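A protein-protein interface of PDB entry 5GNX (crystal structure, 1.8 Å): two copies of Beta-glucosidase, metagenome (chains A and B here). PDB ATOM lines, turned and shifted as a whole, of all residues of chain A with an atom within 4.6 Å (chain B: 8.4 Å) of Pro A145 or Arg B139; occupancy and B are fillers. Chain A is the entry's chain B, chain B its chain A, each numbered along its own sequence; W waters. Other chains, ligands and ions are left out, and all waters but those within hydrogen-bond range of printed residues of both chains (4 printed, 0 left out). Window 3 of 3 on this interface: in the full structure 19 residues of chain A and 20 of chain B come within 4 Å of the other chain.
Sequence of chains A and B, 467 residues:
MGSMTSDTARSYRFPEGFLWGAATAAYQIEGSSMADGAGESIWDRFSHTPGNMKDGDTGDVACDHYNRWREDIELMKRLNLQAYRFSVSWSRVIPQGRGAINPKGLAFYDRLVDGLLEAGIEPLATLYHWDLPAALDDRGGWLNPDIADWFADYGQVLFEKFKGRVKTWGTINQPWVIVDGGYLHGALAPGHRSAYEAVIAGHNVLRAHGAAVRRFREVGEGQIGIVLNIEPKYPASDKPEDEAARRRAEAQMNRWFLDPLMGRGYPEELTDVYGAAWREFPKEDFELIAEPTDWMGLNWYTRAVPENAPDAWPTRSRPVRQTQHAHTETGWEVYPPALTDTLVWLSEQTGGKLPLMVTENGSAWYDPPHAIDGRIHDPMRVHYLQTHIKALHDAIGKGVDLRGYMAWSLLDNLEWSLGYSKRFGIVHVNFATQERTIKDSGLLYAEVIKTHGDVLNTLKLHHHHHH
Water W2 lies within hydrogen-bond range of NE of Arg A139 (2.6 Å), OD1 of Asn B144 (2.8 Å) and OD2 of Asp B146 (3.3 Å).
Water W1 bridges the backbone carbonyl oxygen of Leu B143 (2.8 Å) and the side-chain carboxylate of Asp A138 (2.9 Å).
Water W3 lies within hydrogen-bond range of the guanidinium group (NE) of Arg B139, the side-chain amide oxygen (OD1) of Asn A144 and the side-chain carboxylate (OD2) of Asp A146.
Water W4 bridges the backbone carbonyl oxygen (O) of Leu A143 and the side-chain carboxylate (OD2) of Asp B138.
Hydrophobic or aromatic side chains of chain A within 4 Å of the printed part of chain B: Leu A143 and Pro A145.
Printed residues of chain B that touch a printed residue of chain A: Asp B138, Arg B139, Gly B140, Leu B143, Asn B144 and Pro B145.
Hydrophobic or aromatic side chains of chain B that line the printed part of chain A: Leu B143 and Pro B145.
Asp A138 touches Arg B139, but with the chains exchanged Arg A139 does not touch Asp B138 (4.01 Å).
Asp A138 touches Leu B143, and with the chains exchanged Leu A143 touches Asp B138.
Arg A139 touches Gly B140, and with the chains exchanged Gly A140 touches Arg B139.
Arg A139 touches Pro B145, and with the chains exchanged Pro A145 touches Arg B139.
Positions printed for both chains: 138, 139, 140, 143, 144, 145, 146 and 147.
The backbone carbonyl oxygen (O) of Asp A138 sits close to the backbone carbonyl oxygen (O) of Leu B143, 3.5 Å away.
The backbone NH (N) of Asn A144 sits at hydrogen-bond distance from the backbone carbonyl oxygen (O) of Asp B138, at 3.2 Å.
O of Leu A143 sits close to O of Asp B138.
The backbone NH of Gly A140 lies close to the backbone NH of Gly B140, at 3.4 Å.
O of Arg B139 sits close to O of Arg A139 (3.2 Å).
N of Asn B144 is in hydrogen-bond range of O of Asp A138 (3.3 Å).
The side-chain amide oxygen (OD1) of Asn A144 lies within hydrogen-bond range of the backbone NH (N) of Asp A146 (2.9 Å).
The backbone carbonyl oxygen of Ala B135 lies within hydrogen-bond range of the guanidinium group of Arg B139 (2.8 Å).
The backbone carbonyl oxygen of Arg B139 is in hydrogen-bond range of the side-chain amide nitrogen of Asn B144, at 2.8 Å.
OD1 of Asn B144 lies within hydrogen-bond range of N of Asp B146 (2.9 Å).
The side-chain carboxylate (OD1) of Asp B138 lies within salt-bridge range of the guanidinium group (NH1) of Arg B45 (2.8 Å).
O of Pro A145 sits at hydrogen-bond distance from NH1 of Arg A207 (2.9 Å).
Among the printed residues, merely in contact across the chains: Asp A138 with Arg B139, Asp A138 with Gly B140, Arg A139 with Gly B140, Arg A139 with Asn B144, Arg A139 with Pro B145, Gly A140 with Asp B138, Gly A140 with Arg B139, Asn A144 with Arg B139 and Pro A145 with Arg B139.
Printed residues of chain B within 4 Å of Asp A138: Arg B139 (3.9 Å), Gly B140 (3.3 Å), Leu B143 (3.3 Å) and Asn B144 (3.3 Å).
Of the printed residues of chain B, Arg A139 touches Arg B139, Gly B140, Asn B144 and Pro B145.
Asn A144 touches just these residues of chain B: Asp B138 (3.2 Å) and Arg B139 (3.9 Å).
Of chain B, only Arg B139 comes within 4 Å of Pro A145.
Printed residues of chain A within 4 Å of Arg B139: Asp A138 (3.9 Å), Arg A139 (3.2 Å), Gly A140 (3.6 Å), Asn A144 (3.9 Å) and Pro A145 (3.7 Å).
Printed residues of chain A within 4 Å of Gly B140: Asp A138 (3.3 Å), Arg A139 (3.6 Å) and Gly A140 (3.4 Å).
The nearest residue of chain B that does not touch Pro A145 is Asp B138 (5.2 Å).
The nearest printed residue of chain A that does not touch Arg B139 is Leu A143 (5.4 Å).
The nearest printed residue of chain A that does not touch Leu B143 is Arg A139 (5.3 Å).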
ATOM      1  N   ASP A 138      -0.916 -23.267   7.829  1.00  0.00           N
ATOM      2  CA  ASP A 138      -0.208 -23.795   9.013  1.00  0.00           C
ATOM      3  C   ASP A 138       1.193 -23.233   9.107  1.00  0.00           C
ATOM      4  O   ASP A 138       1.827 -23.327  10.170  1.00  0.00           O
ATOM      5  CB  ASP A 138      -0.140 -25.322   8.979  1.00  0.00           C
ATOM      6  CG  ASP A 138      -1.476 -25.985   9.206  1.00  0.00           C
ATOM      7  OD1 ASP A 138      -2.441 -25.301   9.557  1.00  0.00           O
ATOM      8  OD2 ASP A 138      -1.580 -27.236   9.000  1.00  0.00           O
ATOM      9  N   ARG A 139       1.683 -22.620   8.044  1.00  0.00           N
ATOM     10  CA  ARG A 139       2.953 -21.940   8.056  1.00  0.00           C
ATOM     11  C   ARG A 139       2.792 -20.412   8.007  1.00  0.00           C
ATOM     12  O   ARG A 139       3.715 -19.719   7.705  1.00  0.00           O
ATOM     13  CB  ARG A 139       3.883 -22.453   6.974  1.00  0.00           C
ATOM     14  CG  ARG A 139       4.327 -23.880   7.299  1.00  0.00           C
ATOM     15  CD  ARG A 139       4.763 -24.649   6.108  1.00  0.00           C
ATOM     16  NE  ARG A 139       5.262 -25.933   6.605  1.00  0.00           N
ATOM     17  CZ  ARG A 139       4.511 -27.004   6.761  1.00  0.00           C
ATOM     18  NH1 ARG A 139       3.187 -26.994   6.514  1.00  0.00           N
ATOM     19  NH2 ARG A 139       5.089 -28.111   7.184  1.00  0.00           N
ATOM     20  N   GLY A 140       1.610 -19.963   8.387  1.00  0.00           N
ATOM     21  CA  GLY A 140       1.321 -18.556   8.573  1.00  0.00           C
ATOM     22  C   GLY A 140       0.495 -17.895   7.500  1.00  0.00           C
ATOM     23  O   GLY A 140       0.043 -16.749   7.663  1.00  0.00           O
ATOM     24  N   LEU A 143       0.453 -14.244   6.319  1.00  0.00           N
ATOM     25  CA  LEU A 143       1.307 -13.537   7.276  1.00  0.00           C
ATOM     26  C   LEU A 143       2.807 -13.822   7.099  1.00  0.00           C
ATOM     27  O   LEU A 143       3.654 -13.099   7.651  1.00  0.00           O
ATOM     28  CB  LEU A 143       0.893 -13.858   8.689  1.00  0.00           C
ATOM     29  CG  LEU A 143      -0.586 -13.620   9.053  1.00  0.00           C
ATOM     30  CD1 LEU A 143      -0.782 -13.964  10.497  1.00  0.00           C
ATOM     31  CD2 LEU A 143      -1.012 -12.176   8.758  1.00  0.00           C
ATOM     32  N   ASN A 144       3.116 -14.871   6.379  1.00  0.00           N
ATOM     33  CA  ASN A 144       4.490 -15.304   6.164  1.00  0.00           C
ATOM     34  C   ASN A 144       5.004 -14.678   4.905  1.00  0.00           C
ATOM     35  O   ASN A 144       4.460 -14.926   3.820  1.00  0.00           O
ATOM     36  CB  ASN A 144       4.534 -16.833   6.104  1.00  0.00           C
ATOM     37  CG  ASN A 144       5.958 -17.384   6.063  1.00  0.00           C
ATOM     38  OD1 ASN A 144       6.891 -16.731   5.583  1.00  0.00           O
ATOM     39  ND2 ASN A 144       6.129 -18.561   6.579  1.00  0.00           N
ATOM     40  N   PRO A 145       6.031 -13.837   5.012  1.00  0.00           N
ATOM     41  CA  PRO A 145       6.533 -13.171   3.798  1.00  0.00           C
ATOM     42  C   PRO A 145       7.015 -14.145   2.704  1.00  0.00           C
ATOM     43  O   PRO A 145       7.013 -13.761   1.503  1.00  0.00           O
ATOM     44  CB  PRO A 145       7.687 -12.317   4.330  1.00  0.00           C
ATOM     45  CG  PRO A 145       8.166 -13.066   5.498  1.00  0.00           C
ATOM     46  CD  PRO A 145       6.902 -13.582   6.173  1.00  0.00           C
ATOM     47  N   ASP A 146       7.362 -15.373   3.059  1.00  0.00           N
ATOM     48  CA  ASP A 146       7.737 -16.365   2.058  1.00  0.00           C
ATOM     49  C   ASP A 146       6.597 -16.692   1.093  1.00  0.00           C
ATOM     50  O   ASP A 146       6.845 -17.314   0.036  1.00  0.00           O
ATOM     51  CB  ASP A 146       8.206 -17.668   2.672  1.00  0.00           C
ATOM     52  CG  ASP A 146       9.512 -17.537   3.405  1.00  0.00           C
ATOM     53  OD1 ASP A 146      10.087 -16.444   3.360  1.00  0.00           O
ATOM     54  OD2 ASP A 146       9.930 -18.531   4.039  1.00  0.00           O
ATOM     55  N   ILE A 147       5.374 -16.319   1.450  1.00  0.00           N
ATOM     56  CA  ILE A 147       4.242 -16.660   0.555  1.00  0.00           C
ATOM     57  C   ILE A 147       4.393 -16.010  -0.801  1.00  0.00           C
ATOM     58  O   ILE A 147       3.806 -16.496  -1.789  1.00  0.00           O
ATOM     59  CB  ILE A 147       2.866 -16.283   1.216  1.00  0.00           C
ATOM     60  CG1 ILE A 147       1.698 -16.869   0.392  1.00  0.00           C
ATOM     61  CG2 ILE A 147       2.706 -14.776   1.376  1.00  0.00           C
ATOM     62  CD1 ILE A 147       0.457 -17.112   1.170  1.00  0.00           C
ATOM     63  N   ALA A 148       5.081 -14.868  -0.893  1.00  0.00           N
ATOM     64  CA  ALA A 148       5.333 -14.287  -2.233  1.00  0.00           C
ATOM     65  C   ALA A 148       6.008 -15.316  -3.141  1.00  0.00           C
ATOM     66  O   ALA A 148       5.623 -15.480  -4.303  1.00  0.00           O
ATOM     67  CB  ALA A 148       6.205 -13.050  -2.097  1.00  0.00           C
ATOM     68  N   ASN A 204       1.589  -8.712   2.092  1.00  0.00           N
ATOM     69  CA  ASN A 204       2.091  -9.911   1.455  1.00  0.00           C
ATOM     70  C   ASN A 204       1.259 -10.323   0.259  1.00  0.00           C
ATOM     71  O   ASN A 204       1.803 -10.840  -0.715  1.00  0.00           O
ATOM     72  CB  ASN A 204       2.220 -11.047   2.448  1.00  0.00           C
ATOM     73  CG  ASN A 204       3.395 -10.855   3.365  1.00  0.00           C
ATOM     74  OD1 ASN A 204       4.415 -10.296   2.932  1.00  0.00           O
ATOM     75  ND2 ASN A 204       3.253 -11.230   4.643  1.00  0.00           N
ATOM     76  N   ARG A 207       2.753  -8.220  -2.424  1.00  0.00           N
ATOM     77  CA  ARG A 207       4.055  -8.749  -2.805  1.00  0.00           C
ATOM     78  C   ARG A 207       3.923 -10.012  -3.626  1.00  0.00           C
ATOM     79  O   ARG A 207       4.666 -10.204  -4.619  1.00  0.00           O
ATOM     80  CB  ARG A 207       4.911  -9.024  -1.557  1.00  0.00           C
ATOM     81  CG  ARG A 207       5.377  -7.771  -0.828  1.00  0.00           C
ATOM     82  CD  ARG A 207       6.212  -8.160   0.457  1.00  0.00           C
ATOM     83  NE  ARG A 207       7.360  -8.962   0.087  1.00  0.00           N
ATOM     84  CZ  ARG A 207       7.498 -10.290   0.311  1.00  0.00           C
ATOM     85  NH1 ARG A 207       6.605 -10.954   0.987  1.00  0.00           N
ATOM     86  NH2 ARG A 207       8.603 -10.923  -0.130  1.00  0.00           N
ATOM     87  N   ARG B  45      -0.697  -8.240  20.611  1.00  0.00           N
ATOM     88  CA  ARG B  45      -1.656  -8.014  19.567  1.00  0.00           C
ATOM     89  C   ARG B  45      -3.124  -8.240  20.038  1.00  0.00           C
ATOM     90  O   ARG B  45      -3.992  -7.423  19.794  1.00  0.00           O
ATOM     91  CB  ARG B  45      -1.411  -8.957  18.401  1.00  0.00           C
ATOM     92  CG  ARG B  45      -0.216  -8.586  17.542  1.00  0.00           C
ATOM     93  CD  ARG B  45      -0.015  -9.652  16.485  1.00  0.00           C
ATOM     94  NE  ARG B  45       1.054  -9.308  15.533  1.00  0.00           N
ATOM     95  CZ  ARG B  45       1.411 -10.094  14.508  1.00  0.00           C
ATOM     96  NH1 ARG B  45       0.855 -11.301  14.354  1.00  0.00           N
ATOM     97  NH2 ARG B  45       2.371  -9.704  13.697  1.00  0.00           N
ATOM     98  N   GLN B  96      12.469 -11.805  17.687  1.00  0.00           N
ATOM     99  CA  GLN B  96      11.819 -12.384  16.493  1.00  0.00           C
ATOM    100  C   GLN B  96      11.562 -13.870  16.642  1.00  0.00           C
ATOM    101  O   GLN B  96      11.166 -14.504  15.670  1.00  0.00           O
ATOM    102  CB  GLN B  96      12.641 -12.098  15.245  1.00  0.00           C
ATOM    103  CG  GLN B  96      12.789 -10.601  14.980  1.00  0.00           C
ATOM    104  CD  GLN B  96      11.446  -9.930  14.762  1.00  0.00           C
ATOM    105  OE1 GLN B  96      11.041  -9.029  15.507  1.00  0.00           O
ATOM    106  NE2 GLN B  96      10.737 -10.386  13.763  1.00  0.00           N
ATOM    107  N   GLY B  97      11.747 -14.433  17.842  1.00  0.00           N
ATOM    108  CA  GLY B  97      11.398 -15.829  18.093  1.00  0.00           C
ATOM    109  C   GLY B  97      12.548 -16.757  17.704  1.00  0.00           C
ATOM    110  O   GLY B  97      12.813 -17.769  18.383  1.00  0.00           O
ATOM    111  N   ARG B  98      13.226 -16.397  16.612  1.00  0.00           N
ATOM    112  CA  ARG B  98      14.455 -17.039  16.135  1.00  0.00           C
ATOM    113  C   ARG B  98      15.509 -15.957  15.919  1.00  0.00           C
ATOM    114  O   ARG B  98      15.192 -14.795  15.876  1.00  0.00           O
ATOM    115  CB  ARG B  98      14.253 -17.767  14.819  1.00  0.00           C
ATOM    116  CG  ARG B  98      13.109 -18.717  14.769  1.00  0.00           C
ATOM    117  CD  ARG B  98      12.594 -18.726  13.341  1.00  0.00           C
ATOM    118  NE  ARG B  98      13.308 -19.744  12.633  1.00  0.00           N
ATOM    119  CZ  ARG B  98      13.218 -19.986  11.333  1.00  0.00           C
ATOM    120  NH1 ARG B  98      12.464 -19.205  10.586  1.00  0.00           N
ATOM    121  NH2 ARG B  98      13.891 -21.034  10.817  1.00  0.00           N
ATOM    122  N   LEU B 132       3.650 -16.569  22.808  1.00  0.00           N
ATOM    123  CA  LEU B 132       4.401 -16.766  21.594  1.00  0.00           C
ATOM    124  C   LEU B 132       4.821 -15.434  20.953  1.00  0.00           C
ATOM    125  O   LEU B 132       3.993 -14.525  20.826  1.00  0.00           O
ATOM    126  CB  LEU B 132       3.573 -17.566  20.606  1.00  0.00           C
ATOM    127  CG  LEU B 132       4.331 -18.098  19.422  1.00  0.00           C
ATOM    128  CD1 LEU B 132       5.284 -19.179  19.872  1.00  0.00           C
ATOM    129  CD2 LEU B 132       3.306 -18.667  18.458  1.00  0.00           C
ATOM    130  N   PRO B 133       6.093 -15.309  20.495  1.00  0.00           N
ATOM    131  CA  PRO B 133       6.463 -14.131  19.699  1.00  0.00           C
ATOM    132  C   PRO B 133       5.596 -14.009  18.448  1.00  0.00           C
ATOM    133  O   PRO B 133       5.328 -14.994  17.766  1.00  0.00           O
ATOM    134  CB  PRO B 133       7.926 -14.411  19.294  1.00  0.00           C
ATOM    135  CG  PRO B 133       8.454 -15.319  20.421  1.00  0.00           C
ATOM    136  CD  PRO B 133       7.241 -16.221  20.724  1.00  0.00           C
ATOM    137  N   ALA B 134       5.168 -12.803  18.151  1.00  0.00           N
ATOM    138  CA  ALA B 134       4.297 -12.606  17.013  1.00  0.00           C
ATOM    139  C   ALA B 134       4.972 -12.937  15.702  1.00  0.00           C
ATOM    140  O   ALA B 134       4.317 -13.374  14.758  1.00  0.00           O
ATOM    141  CB  ALA B 134       3.772 -11.190  16.998  1.00  0.00           C
ATOM    142  N   ALA B 135       6.284 -12.734  15.624  1.00  0.00           N
ATOM    143  CA  ALA B 135       7.045 -13.148  14.424  1.00  0.00           C
ATOM    144  C   ALA B 135       6.878 -14.646  14.155  1.00  0.00           C
ATOM    145  O   ALA B 135       6.897 -15.073  13.022  1.00  0.00           O
ATOM    146  CB  ALA B 135       8.487 -12.805  14.574  1.00  0.00           C
ATOM    147  N   LEU B 136       6.704 -15.463  15.202  1.00  0.00           N
ATOM    148  CA  LEU B 136       6.506 -16.884  14.974  1.00  0.00           C
ATOM    149  C   LEU B 136       5.044 -17.219  14.661  1.00  0.00           C
ATOM    150  O   LEU B 136       4.768 -18.119  13.883  1.00  0.00           O
ATOM    151  CB  LEU B 136       7.035 -17.714  16.144  1.00  0.00           C
ATOM    152  CG  LEU B 136       8.518 -17.571  16.463  1.00  0.00           C
ATOM    153  CD1 LEU B 136       8.970 -18.471  17.640  1.00  0.00           C
ATOM    154  CD2 LEU B 136       9.379 -17.785  15.211  1.00  0.00           C
ATOM    155  N   ASP B 137       4.125 -16.483  15.244  1.00  0.00           N
ATOM    156  CA  ASP B 137       2.723 -16.615  14.862  1.00  0.00           C
ATOM    157  C   ASP B 137       2.524 -16.299  13.376  1.00  0.00           C
ATOM    158  O   ASP B 137       1.696 -16.952  12.675  1.00  0.00           O
ATOM    159  CB  ASP B 137       1.860 -15.713  15.722  1.00  0.00           C
ATOM    160  CG  ASP B 137       0.388 -16.183  15.762  1.00  0.00           C
ATOM    161  OD1 ASP B 137       0.125 -17.388  16.066  1.00  0.00           O
ATOM    162  OD2 ASP B 137      -0.476 -15.365  15.505  1.00  0.00           O
ATOM    163  N   ASP B 138       3.252 -15.317  12.884  1.00  0.00           N
ATOM    164  CA  ASP B 138       3.211 -14.967  11.455  1.00  0.00           C
ATOM    165  C   ASP B 138       3.790 -16.084  10.571  1.00  0.00           C
ATOM    166  O   ASP B 138       3.588 -16.065   9.360  1.00  0.00           O
ATOM    167  CB  ASP B 138       3.974 -13.669  11.194  1.00  0.00           C
ATOM    168  CG  ASP B 138       3.299 -12.443  11.768  1.00  0.00           C
ATOM    169  OD1 ASP B 138       2.120 -12.544  12.225  1.00  0.00           O
ATOM    170  OD2 ASP B 138       3.941 -11.373  11.790  1.00  0.00           O
ATOM    171  N   ARG B 139       4.433 -17.092  11.180  1.00  0.00           N
ATOM    172  CA  ARG B 139       4.961 -18.250  10.476  1.00  0.00           C
ATOM    173  C   ARG B 139       4.173 -19.514  10.890  1.00  0.00           C
ATOM    174  O   ARG B 139       4.612 -20.628  10.687  1.00  0.00           O
ATOM    175  CB  ARG B 139       6.462 -18.384  10.725  1.00  0.00           C
ATOM    176  CG  ARG B 139       7.193 -17.196  10.077  1.00  0.00           C
ATOM    177  CD  ARG B 139       8.618 -16.966  10.471  1.00  0.00           C
ATOM    178  NE  ARG B 139       9.145 -15.906   9.567  1.00  0.00           N
ATOM    179  CZ  ARG B 139       9.011 -14.593   9.745  1.00  0.00           C
ATOM    180  NH1 ARG B 139       8.343 -14.066  10.798  1.00  0.00           N
ATOM    181  NH2 ARG B 139       9.569 -13.789   8.835  1.00  0.00           N
ATOM    182  N   GLY B 140       2.967 -19.283  11.439  1.00  0.00           N
ATOM    183  CA  GLY B 140       2.041 -20.372  11.718  1.00  0.00           C
ATOM    184  C   GLY B 140       1.911 -20.735  13.185  1.00  0.00           C
ATOM    185  O   GLY B 140       1.057 -21.523  13.555  1.00  0.00           O
ATOM    186  N   GLY B 141       2.833 -20.217  13.993  1.00  0.00           N
ATOM    187  CA  GLY B 141       2.817 -20.502  15.407  1.00  0.00           C
ATOM    188  C   GLY B 141       2.783 -21.968  15.708  1.00  0.00           C
ATOM    189  O   GLY B 141       3.538 -22.727  15.140  1.00  0.00           O
ATOM    190  N   TRP B 142       1.888 -22.392  16.591  1.00  0.00           N
ATOM    191  CA  TRP B 142       1.831 -23.815  16.979  1.00  0.00           C
ATOM    192  C   TRP B 142       1.308 -24.724  15.879  1.00  0.00           C
ATOM    193  O   TRP B 142       1.283 -25.949  16.050  1.00  0.00           O
ATOM    194  CB  TRP B 142       0.983 -23.975  18.273  1.00  0.00           C
ATOM    195  CG  TRP B 142       1.647 -23.316  19.410  1.00  0.00           C
ATOM    196  CD1 TRP B 142       1.295 -22.142  20.017  1.00  0.00           C
ATOM    197  CD2 TRP B 142       2.833 -23.789  20.093  1.00  0.00           C
ATOM    198  NE1 TRP B 142       2.198 -21.849  21.030  1.00  0.00           N
ATOM    199  CE2 TRP B 142       3.145 -22.835  21.084  1.00  0.00           C
ATOM    200  CE3 TRP B 142       3.654 -24.930  19.940  1.00  0.00           C
ATOM    201  CZ2 TRP B 142       4.250 -22.976  21.932  1.00  0.00           C
ATOM    202  CZ3 TRP B 142       4.763 -25.070  20.770  1.00  0.00           C
ATOM    203  CH2 TRP B 142       5.045 -24.105  21.756  1.00  0.00           C
ATOM    204  N   LEU B 143       0.876 -24.177  14.730  1.00  0.00           N
ATOM    205  CA  LEU B 143       0.529 -25.005  13.602  1.00  0.00           C
ATOM    206  C   LEU B 143       1.719 -25.430  12.741  1.00  0.00           C
ATOM    207  O   LEU B 143       1.589 -26.314  11.891  1.00  0.00           O
ATOM    208  CB  LEU B 143      -0.479 -24.306  12.704  1.00  0.00           C
ATOM    209  CG  LEU B 143      -1.717 -23.785  13.427  1.00  0.00           C
ATOM    210  CD1 LEU B 143      -2.626 -23.107  12.418  1.00  0.00           C
ATOM    211  CD2 LEU B 143      -2.385 -24.956  14.102  1.00  0.00           C
ATOM    212  N   ASN B 144       2.840 -24.775  12.913  1.00  0.00           N
ATOM    213  CA  ASN B 144       4.011 -25.069  12.102  1.00  0.00           C
ATOM    214  C   ASN B 144       4.888 -26.089  12.807  1.00  0.00           C
ATOM    215  O   ASN B 144       5.357 -25.843  13.924  1.00  0.00           O
ATOM    216  CB  ASN B 144       4.796 -23.766  11.832  1.00  0.00           C
ATOM    217  CG  ASN B 144       5.928 -23.943  10.869  1.00  0.00           C
ATOM    218  OD1 ASN B 144       6.473 -25.039  10.707  1.00  0.00           O
ATOM    219  ND2 ASN B 144       6.332 -22.848  10.236  1.00  0.00           N
ATOM    220  N   PRO B 145       5.082 -27.255  12.193  1.00  0.00           N
ATOM    221  CA  PRO B 145       5.870 -28.298  12.873  1.00  0.00           C
ATOM    222  C   PRO B 145       7.268 -27.835  13.274  1.00  0.00           C
ATOM    223  O   PRO B 145       7.843 -28.354  14.265  1.00  0.00           O
ATOM    224  CB  PRO B 145       5.975 -29.406  11.822  1.00  0.00           C
ATOM    225  CG  PRO B 145       5.630 -28.818  10.554  1.00  0.00           C
ATOM    226  CD  PRO B 145       4.685 -27.659  10.845  1.00  0.00           C
ATOM    227  N   ASP B 146       7.813 -26.846  12.590  1.00  0.00           N
ATOM    228  CA  ASP B 146       9.146 -26.369  12.934  1.00  0.00           C
ATOM    229  C   ASP B 146       9.196 -25.707  14.315  1.00  0.00           C
ATOM    230  O   ASP B 146      10.285 -25.480  14.857  1.00  0.00           O
ATOM    231  CB  ASP B 146       9.640 -25.356  11.914  1.00  0.00           C
ATOM    232  CG  ASP B 146       9.903 -25.966  10.544  1.00  0.00           C
ATOM    233  OD1 ASP B 146       9.926 -27.213  10.413  1.00  0.00           O
ATOM    234  OD2 ASP B 146      10.093 -25.157   9.606  1.00  0.00           O
ATOM    235  N   ILE B 147       8.040 -25.399  14.890  1.00  0.00           N
ATOM    236  CA  ILE B 147       8.011 -24.737  16.196  1.00  0.00           C
ATOM    237  C   ILE B 147       8.690 -25.606  17.250  1.00  0.00           C
ATOM    238  O   ILE B 147       9.207 -25.063  18.233  1.00  0.00           O
ATOM    239  CB  ILE B 147       6.575 -24.382  16.661  1.00  0.00           C
ATOM    240  CG1 ILE B 147       6.644 -23.417  17.861  1.00  0.00           C
ATOM    241  CG2 ILE B 147       5.715 -25.639  16.997  1.00  0.00           C
ATOM    242  CD1 ILE B 147       5.517 -22.477  17.955  1.00  0.00           C
ATOM    243  N   TRP B 150      12.225 -24.508  16.946  1.00  0.00           N
ATOM    244  CA  TRP B 150      12.357 -23.118  17.388  1.00  0.00           C
ATOM    245  C   TRP B 150      12.300 -23.046  18.944  1.00  0.00           C
ATOM    246  O   TRP B 150      13.062 -22.309  19.560  1.00  0.00           O
ATOM    247  CB  TRP B 150      11.252 -22.270  16.825  1.00  0.00           C
ATOM    248  CG  TRP B 150      11.209 -22.240  15.365  1.00  0.00           C
ATOM    249  CD1 TRP B 150      12.208 -22.525  14.526  1.00  0.00           C
ATOM    250  CD2 TRP B 150      10.072 -21.883  14.545  1.00  0.00           C
ATOM    251  NE1 TRP B 150      11.769 -22.380  13.205  1.00  0.00           N
ATOM    252  CE2 TRP B 150      10.480 -21.977  13.217  1.00  0.00           C
ATOM    253  CE3 TRP B 150       8.780 -21.519  14.830  1.00  0.00           C
ATOM    254  CZ2 TRP B 150       9.600 -21.705  12.146  1.00  0.00           C
ATOM    255  CZ3 TRP B 150       7.911 -21.267  13.782  1.00  0.00           C
ATOM    256  CH2 TRP B 150       8.337 -21.382  12.484  1.00  0.00           C
HETATM  257  O   HOH W   1       0.824 -28.357  10.133  1.00  0.00           O
HETATM  258  O   HOH W   2       7.258 -26.133   8.256  1.00  0.00           O
HETATM  259  O   HOH W   3       9.423 -16.484   6.818  1.00  0.00           O
HETATM  260  O   HOH W   4       5.142 -11.192   9.118  1.00  0.00           O
